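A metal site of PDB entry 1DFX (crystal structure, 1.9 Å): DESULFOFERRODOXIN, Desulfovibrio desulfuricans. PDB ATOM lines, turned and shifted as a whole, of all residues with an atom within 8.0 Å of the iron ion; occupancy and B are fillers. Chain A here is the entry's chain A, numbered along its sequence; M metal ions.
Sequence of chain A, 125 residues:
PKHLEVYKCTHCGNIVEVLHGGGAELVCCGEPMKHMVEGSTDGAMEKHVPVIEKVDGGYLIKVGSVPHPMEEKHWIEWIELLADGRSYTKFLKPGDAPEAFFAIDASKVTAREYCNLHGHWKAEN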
ATOM      1  N   GLY A  43      -1.953  -7.933  33.820  1.00  0.00           N
ATOM      2  CA  GLY A  43      -0.881  -7.618  32.890  1.00  0.00           C
ATOM      3  C   GLY A  43      -1.392  -6.698  31.780  1.00  0.00           C
ATOM      4  O   GLY A  43      -1.692  -5.540  32.055  1.00  0.00           O
ATOM      5  N   ALA A  44      -1.519  -7.236  30.584  1.00  0.00           N
ATOM      6  CA  ALA A  44      -1.993  -6.509  29.431  1.00  0.00           C
ATOM      7  C   ALA A  44      -3.144  -7.205  28.733  1.00  0.00           C
ATOM      8  O   ALA A  44      -2.967  -8.069  27.862  1.00  0.00           O
ATOM      9  CB  ALA A  44      -0.854  -6.245  28.447  1.00  0.00           C
ATOM     10  N   LYS A  47      -2.649  -7.916  25.250  1.00  0.00           N
ATOM     11  CA  LYS A  47      -1.630  -8.874  24.872  1.00  0.00           C
ATOM     12  C   LYS A  47      -1.702 -10.186  25.577  1.00  0.00           C
ATOM     13  O   LYS A  47      -0.954 -11.126  25.231  1.00  0.00           O
ATOM     14  CB  LYS A  47      -0.239  -8.269  24.907  1.00  0.00           C
ATOM     15  CG  LYS A  47      -0.205  -6.746  24.946  1.00  0.00           C
ATOM     16  CD  LYS A  47       1.211  -6.242  25.179  1.00  0.00           C
ATOM     17  CE  LYS A  47       1.721  -5.469  23.972  1.00  0.00           C
ATOM     18  NZ  LYS A  47       3.209  -5.484  23.902  1.00  0.00           N
ATOM     19  N   HIS A  48      -2.546 -10.322  26.593  1.00  0.00           N
ATOM     20  CA  HIS A  48      -2.549 -11.602  27.324  1.00  0.00           C
ATOM     21  C   HIS A  48      -3.844 -12.356  27.189  1.00  0.00           C
ATOM     22  O   HIS A  48      -3.858 -13.594  27.174  1.00  0.00           O
ATOM     23  CB  HIS A  48      -2.206 -11.358  28.797  1.00  0.00           C
ATOM     24  CG  HIS A  48      -0.791 -10.887  28.973  1.00  0.00           C
ATOM     25  ND1 HIS A  48      -0.474  -9.639  29.462  1.00  0.00           N
ATOM     26  CD2 HIS A  48       0.386 -11.512  28.676  1.00  0.00           C
ATOM     27  CE1 HIS A  48       0.850  -9.516  29.476  1.00  0.00           C
ATOM     28  NE2 HIS A  48       1.386 -10.626  29.006  1.00  0.00           N
ATOM     29  N   VAL A  63      -2.547 -15.041  20.946  1.00  0.00           N
ATOM     30  CA  VAL A  63      -2.440 -14.228  22.209  1.00  0.00           C
ATOM     31  C   VAL A  63      -1.648 -12.954  21.807  1.00  0.00           C
ATOM     32  O   VAL A  63      -0.492 -13.128  21.412  1.00  0.00           O
ATOM     33  CB  VAL A  63      -1.513 -15.008  23.197  1.00  0.00           C
ATOM     34  CG1 VAL A  63      -1.481 -14.297  24.532  1.00  0.00           C
ATOM     35  CG2 VAL A  63      -2.019 -16.427  23.336  1.00  0.00           C
ATOM     36  N   HIS A  68       1.573 -11.042  21.278  1.00  0.00           N
ATOM     37  CA  HIS A  68       2.381 -10.874  22.521  1.00  0.00           C
ATOM     38  C   HIS A  68       3.821 -11.236  22.127  1.00  0.00           C
ATOM     39  O   HIS A  68       4.028 -12.068  21.231  1.00  0.00           O
ATOM     40  CB  HIS A  68       1.878 -11.926  23.544  1.00  0.00           C
ATOM     41  CG  HIS A  68       2.547 -11.894  24.870  1.00  0.00           C
ATOM     42  ND1 HIS A  68       3.790 -12.416  25.103  1.00  0.00           N
ATOM     43  CD2 HIS A  68       2.093 -11.440  26.076  1.00  0.00           C
ATOM     44  CE1 HIS A  68       4.115 -12.250  26.384  1.00  0.00           C
ATOM     45  NE2 HIS A  68       3.107 -11.667  26.991  1.00  0.00           N
ATOM     46  N   PRO A  69       4.782 -10.596  22.736  1.00  0.00           N
ATOM     47  CA  PRO A  69       6.196 -10.892  22.480  1.00  0.00           C
ATOM     48  C   PRO A  69       6.503 -12.390  22.653  1.00  0.00           C
ATOM     49  O   PRO A  69       5.851 -13.057  23.485  1.00  0.00           O
ATOM     50  CB  PRO A  69       6.894 -10.118  23.608  1.00  0.00           C
ATOM     51  CG  PRO A  69       5.963  -9.040  23.996  1.00  0.00           C
ATOM     52  CD  PRO A  69       4.572  -9.473  23.622  1.00  0.00           C
ATOM     53  N   LYS A  73      13.329 -13.962  27.029  1.00  0.00           N
ATOM     54  CA  LYS A  73      13.015 -13.744  28.423  1.00  0.00           C
ATOM     55  C   LYS A  73      11.581 -13.346  28.661  1.00  0.00           C
ATOM     56  O   LYS A  73      11.183 -13.074  29.802  1.00  0.00           O
ATOM     57  CB  LYS A  73      13.974 -12.726  29.049  1.00  0.00           C
ATOM     58  CG  LYS A  73      15.407 -12.811  28.529  1.00  0.00           C
ATOM     59  CD  LYS A  73      16.232 -13.752  29.385  1.00  0.00           C
ATOM     60  CE  LYS A  73      16.158 -13.374  30.861  1.00  0.00           C
ATOM     61  NZ  LYS A  73      16.827 -12.067  31.132  1.00  0.00           N
ATOM     62  N   HIS A  74      10.774 -13.284  27.599  1.00  0.00           N
ATOM     63  CA  HIS A  74       9.354 -12.923  27.807  1.00  0.00           C
ATOM     64  C   HIS A  74       8.544 -13.543  26.669  1.00  0.00           C
ATOM     65  O   HIS A  74       8.569 -13.054  25.546  1.00  0.00           O
ATOM     66  CB  HIS A  74       9.204 -11.397  27.723  1.00  0.00           C
ATOM     67  CG  HIS A  74       7.798 -10.925  27.917  1.00  0.00           C
ATOM     68  ND1 HIS A  74       7.338  -9.726  27.477  1.00  0.00           N
ATOM     69  CD2 HIS A  74       6.744 -11.521  28.539  1.00  0.00           C
ATOM     70  CE1 HIS A  74       6.054  -9.581  27.814  1.00  0.00           C
ATOM     71  NE2 HIS A  74       5.673 -10.676  28.455  1.00  0.00           N
ATOM     72  N   TRP A  75       7.884 -14.663  26.947  1.00  0.00           N
ATOM     73  CA  TRP A  75       7.147 -15.362  25.889  1.00  0.00           C
ATOM     74  C   TRP A  75       5.963 -16.142  26.477  1.00  0.00           C
ATOM     75  O   TRP A  75       5.901 -16.340  27.689  1.00  0.00           O
ATOM     76  CB  TRP A  75       8.039 -16.279  25.091  1.00  0.00           C
ATOM     77  CG  TRP A  75       8.275 -17.655  25.625  1.00  0.00           C
ATOM     78  CD1 TRP A  75       7.847 -18.827  25.056  1.00  0.00           C
ATOM     79  CD2 TRP A  75       9.020 -18.027  26.787  1.00  0.00           C
ATOM     80  NE1 TRP A  75       8.268 -19.900  25.818  1.00  0.00           N
ATOM     81  CE2 TRP A  75       8.986 -19.438  26.874  1.00  0.00           C
ATOM     82  CE3 TRP A  75       9.714 -17.306  27.765  1.00  0.00           C
ATOM     83  CZ2 TRP A  75       9.606 -20.145  27.909  1.00  0.00           C
ATOM     84  CZ3 TRP A  75      10.331 -18.018  28.787  1.00  0.00           C
ATOM     85  CH2 TRP A  75      10.279 -19.418  28.853  1.00  0.00           C
ATOM     86  N   ILE A  76       5.071 -16.540  25.589  1.00  0.00           N
ATOM     87  CA  ILE A  76       3.898 -17.362  26.019  1.00  0.00           C
ATOM     88  C   ILE A  76       4.349 -18.821  26.016  1.00  0.00           C
ATOM     89  O   ILE A  76       4.748 -19.332  24.969  1.00  0.00           O
ATOM     90  CB  ILE A  76       2.781 -17.179  24.960  1.00  0.00           C
ATOM     91  CG1 ILE A  76       2.434 -15.699  24.758  1.00  0.00           C
ATOM     92  CG2 ILE A  76       1.556 -18.001  25.366  1.00  0.00           C
ATOM     93  CD1 ILE A  76       2.175 -14.957  26.050  1.00  0.00           C
ATOM     94  N   GLU A 113      -3.730 -19.122  28.396  1.00  0.00           N
ATOM     95  CA  GLU A 113      -2.302 -19.058  27.938  1.00  0.00           C
ATOM     96  C   GLU A 113      -1.499 -18.666  29.168  1.00  0.00           C
ATOM     97  O   GLU A 113      -2.008 -18.095  30.141  1.00  0.00           O
ATOM     98  CB  GLU A 113      -2.154 -18.043  26.825  1.00  0.00           C
ATOM     99  CG  GLU A 113      -2.626 -16.638  27.229  1.00  0.00           C
ATOM    100  CD  GLU A 113      -1.444 -15.839  27.766  1.00  0.00           C
ATOM    101  OE1 GLU A 113      -0.362 -16.453  27.855  1.00  0.00           O
ATOM    102  OE2 GLU A 113      -1.617 -14.661  28.111  1.00  0.00           O
ATOM    103  N   TYR A 114      -0.218 -18.977  29.147  1.00  0.00           N
ATOM    104  CA  TYR A 114       0.585 -18.573  30.314  1.00  0.00           C
ATOM    105  C   TYR A 114       1.823 -17.807  29.785  1.00  0.00           C
ATOM    106  O   TYR A 114       2.497 -18.360  28.903  1.00  0.00           O
ATOM    107  CB  TYR A 114       1.087 -19.880  31.003  1.00  0.00           C
ATOM    108  CG  TYR A 114       1.852 -19.489  32.267  1.00  0.00           C
ATOM    109  CD1 TYR A 114       1.172 -19.119  33.403  1.00  0.00           C
ATOM    110  CD2 TYR A 114       3.247 -19.412  32.238  1.00  0.00           C
ATOM    111  CE1 TYR A 114       1.872 -18.720  34.543  1.00  0.00           C
ATOM    112  CE2 TYR A 114       3.940 -19.010  33.372  1.00  0.00           C
ATOM    113  CZ  TYR A 114       3.244 -18.672  34.506  1.00  0.00           C
ATOM    114  OH  TYR A 114       3.934 -18.299  35.642  1.00  0.00           O
ATOM    115  N   CYS A 115       2.004 -16.615  30.295  1.00  0.00           N
ATOM    116  CA  CYS A 115       3.144 -15.758  29.938  1.00  0.00           C
ATOM    117  C   CYS A 115       4.150 -15.840  31.101  1.00  0.00           C
ATOM    118  O   CYS A 115       3.781 -15.642  32.264  1.00  0.00           O
ATOM    119  CB  CYS A 115       2.668 -14.293  29.840  1.00  0.00           C
ATOM    120  SG  CYS A 115       4.038 -13.115  29.694  1.00  0.00           S
ATOM    121  N   ASN A 116       5.388 -16.177  30.780  1.00  0.00           N
ATOM    122  CA  ASN A 116       6.393 -16.318  31.816  1.00  0.00           C
ATOM    123  C   ASN A 116       6.424 -15.197  32.801  1.00  0.00           C
ATOM    124  O   ASN A 116       6.668 -15.391  34.004  1.00  0.00           O
ATOM    125  CB  ASN A 116       7.751 -16.680  31.252  1.00  0.00           C
ATOM    126  CG  ASN A 116       8.391 -15.486  30.547  1.00  0.00           C
ATOM    127  OD1 ASN A 116       7.717 -14.736  29.862  1.00  0.00           O
ATOM    128  ND2 ASN A 116       9.695 -15.334  30.762  1.00  0.00           N
ATOM    129  N   LEU A 117       6.207 -13.944  32.360  1.00  0.00           N
ATOM    130  CA  LEU A 117       6.314 -12.832  33.292  1.00  0.00           C
ATOM    131  C   LEU A 117       4.946 -12.407  33.824  1.00  0.00           C
ATOM    132  O   LEU A 117       4.847 -11.953  34.950  1.00  0.00           O
ATOM    133  CB  LEU A 117       6.899 -11.595  32.543  1.00  0.00           C
ATOM    134  CG  LEU A 117       8.330 -11.687  32.062  1.00  0.00           C
ATOM    135  CD1 LEU A 117       8.816 -10.305  31.598  1.00  0.00           C
ATOM    136  CD2 LEU A 117       9.252 -12.233  33.141  1.00  0.00           C
ATOM    137  N   HIS A 118       3.943 -12.481  32.950  1.00  0.00           N
ATOM    138  CA  HIS A 118       2.629 -12.047  33.186  1.00  0.00           C
ATOM    139  C   HIS A 118       1.640 -12.973  33.745  1.00  0.00           C
ATOM    140  O   HIS A 118       0.523 -12.592  34.137  1.00  0.00           O
ATOM    141  CB  HIS A 118       2.094 -11.015  32.207  1.00  0.00           C
ATOM    142  CG  HIS A 118       3.140  -9.977  31.865  1.00  0.00           C
ATOM    143  ND1 HIS A 118       3.887 -10.025  30.715  1.00  0.00           N
ATOM    144  CD2 HIS A 118       3.623  -8.956  32.609  1.00  0.00           C
ATOM    145  CE1 HIS A 118       4.753  -9.030  30.719  1.00  0.00           C
ATOM    146  NE2 HIS A 118       4.614  -8.359  31.858  1.00  0.00           N
ATOM    147  N   GLY A 119       1.975 -14.284  33.886  1.00  0.00           N
ATOM    148  CA  GLY A 119       1.012 -15.152  34.536  1.00  0.00           C
ATOM    149  C   GLY A 119      -0.044 -15.733  33.629  1.00  0.00           C
ATOM    150  O   GLY A 119       0.129 -15.784  32.410  1.00  0.00           O
ATOM    151  N   TRP A 121      -3.889 -16.369  32.037  1.00  0.00           N
ATOM    152  CA  TRP A 121      -5.040 -15.688  31.491  1.00  0.00           C
ATOM    153  C   TRP A 121      -5.947 -16.641  30.711  1.00  0.00           C
ATOM    154  O   TRP A 121      -5.510 -17.621  30.135  1.00  0.00           O
ATOM    155  CB  TRP A 121      -4.581 -14.609  30.478  1.00  0.00           C
ATOM    156  CG  TRP A 121      -3.593 -13.668  31.097  1.00  0.00           C
ATOM    157  CD1 TRP A 121      -2.258 -13.882  31.261  1.00  0.00           C
ATOM    158  CD2 TRP A 121      -3.876 -12.379  31.648  1.00  0.00           C
ATOM    159  NE1 TRP A 121      -1.688 -12.791  31.879  1.00  0.00           N
ATOM    160  CE2 TRP A 121      -2.654 -11.856  32.129  1.00  0.00           C
ATOM    161  CE3 TRP A 121      -5.033 -11.623  31.779  1.00  0.00           C
ATOM    162  CZ2 TRP A 121      -2.571 -10.609  32.723  1.00  0.00           C
ATOM    163  CZ3 TRP A 121      -4.936 -10.373  32.376  1.00  0.00           C
ATOM    164  CH2 TRP A 121      -3.720  -9.884  32.846  1.00  0.00           C
HETATM  165 FE    FE M   1       3.542 -11.030  28.901  1.00  0.00          FE
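The backbone NH (N) of His 68 is in hydrogen-bond range of the backbone carbonyl oxygen (O) of Val 63.
O of His 118 is in hydrogen-bond range of NE1 of Trp 121 (3.2 Å).
The backbone carbonyl oxygen (O) of His 48 lies close to the side-chain carboxylate (OE2) of Glu 113 (2.7 Å).
ND1 of His 48 sits at hydrogen-bond distance from N of Ala 44 (2.9 Å).
The side-chain sulfur (SG) of Cys 115 sits close to the backbone NH (N) of Leu 117 (3.5 Å).
OE1 of Glu 113 lies within hydrogen-bond range of N of Cys 115, 3.4 Å away.
Five residues have an atom within 4 Å of the iron ion: His 48, His 68, His 74, Cys 115 and His 118.
Along chain A the residues within 4 Å of the iron ion span positions 48 to 118.
The iron ion is bound by NE2 of His 68 (2.1 Å).
The iron ion is bound by ND1 of His 118 (2.1 Å).
A ring nitrogen (NE2) of His 48 is bound to the iron ion, at 2.2 Å.
The iron ion is bound by NE2 of His 74, at 2.2 Å.
The iron ion is bound by SG of Cys 115, 2.3 Å away.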
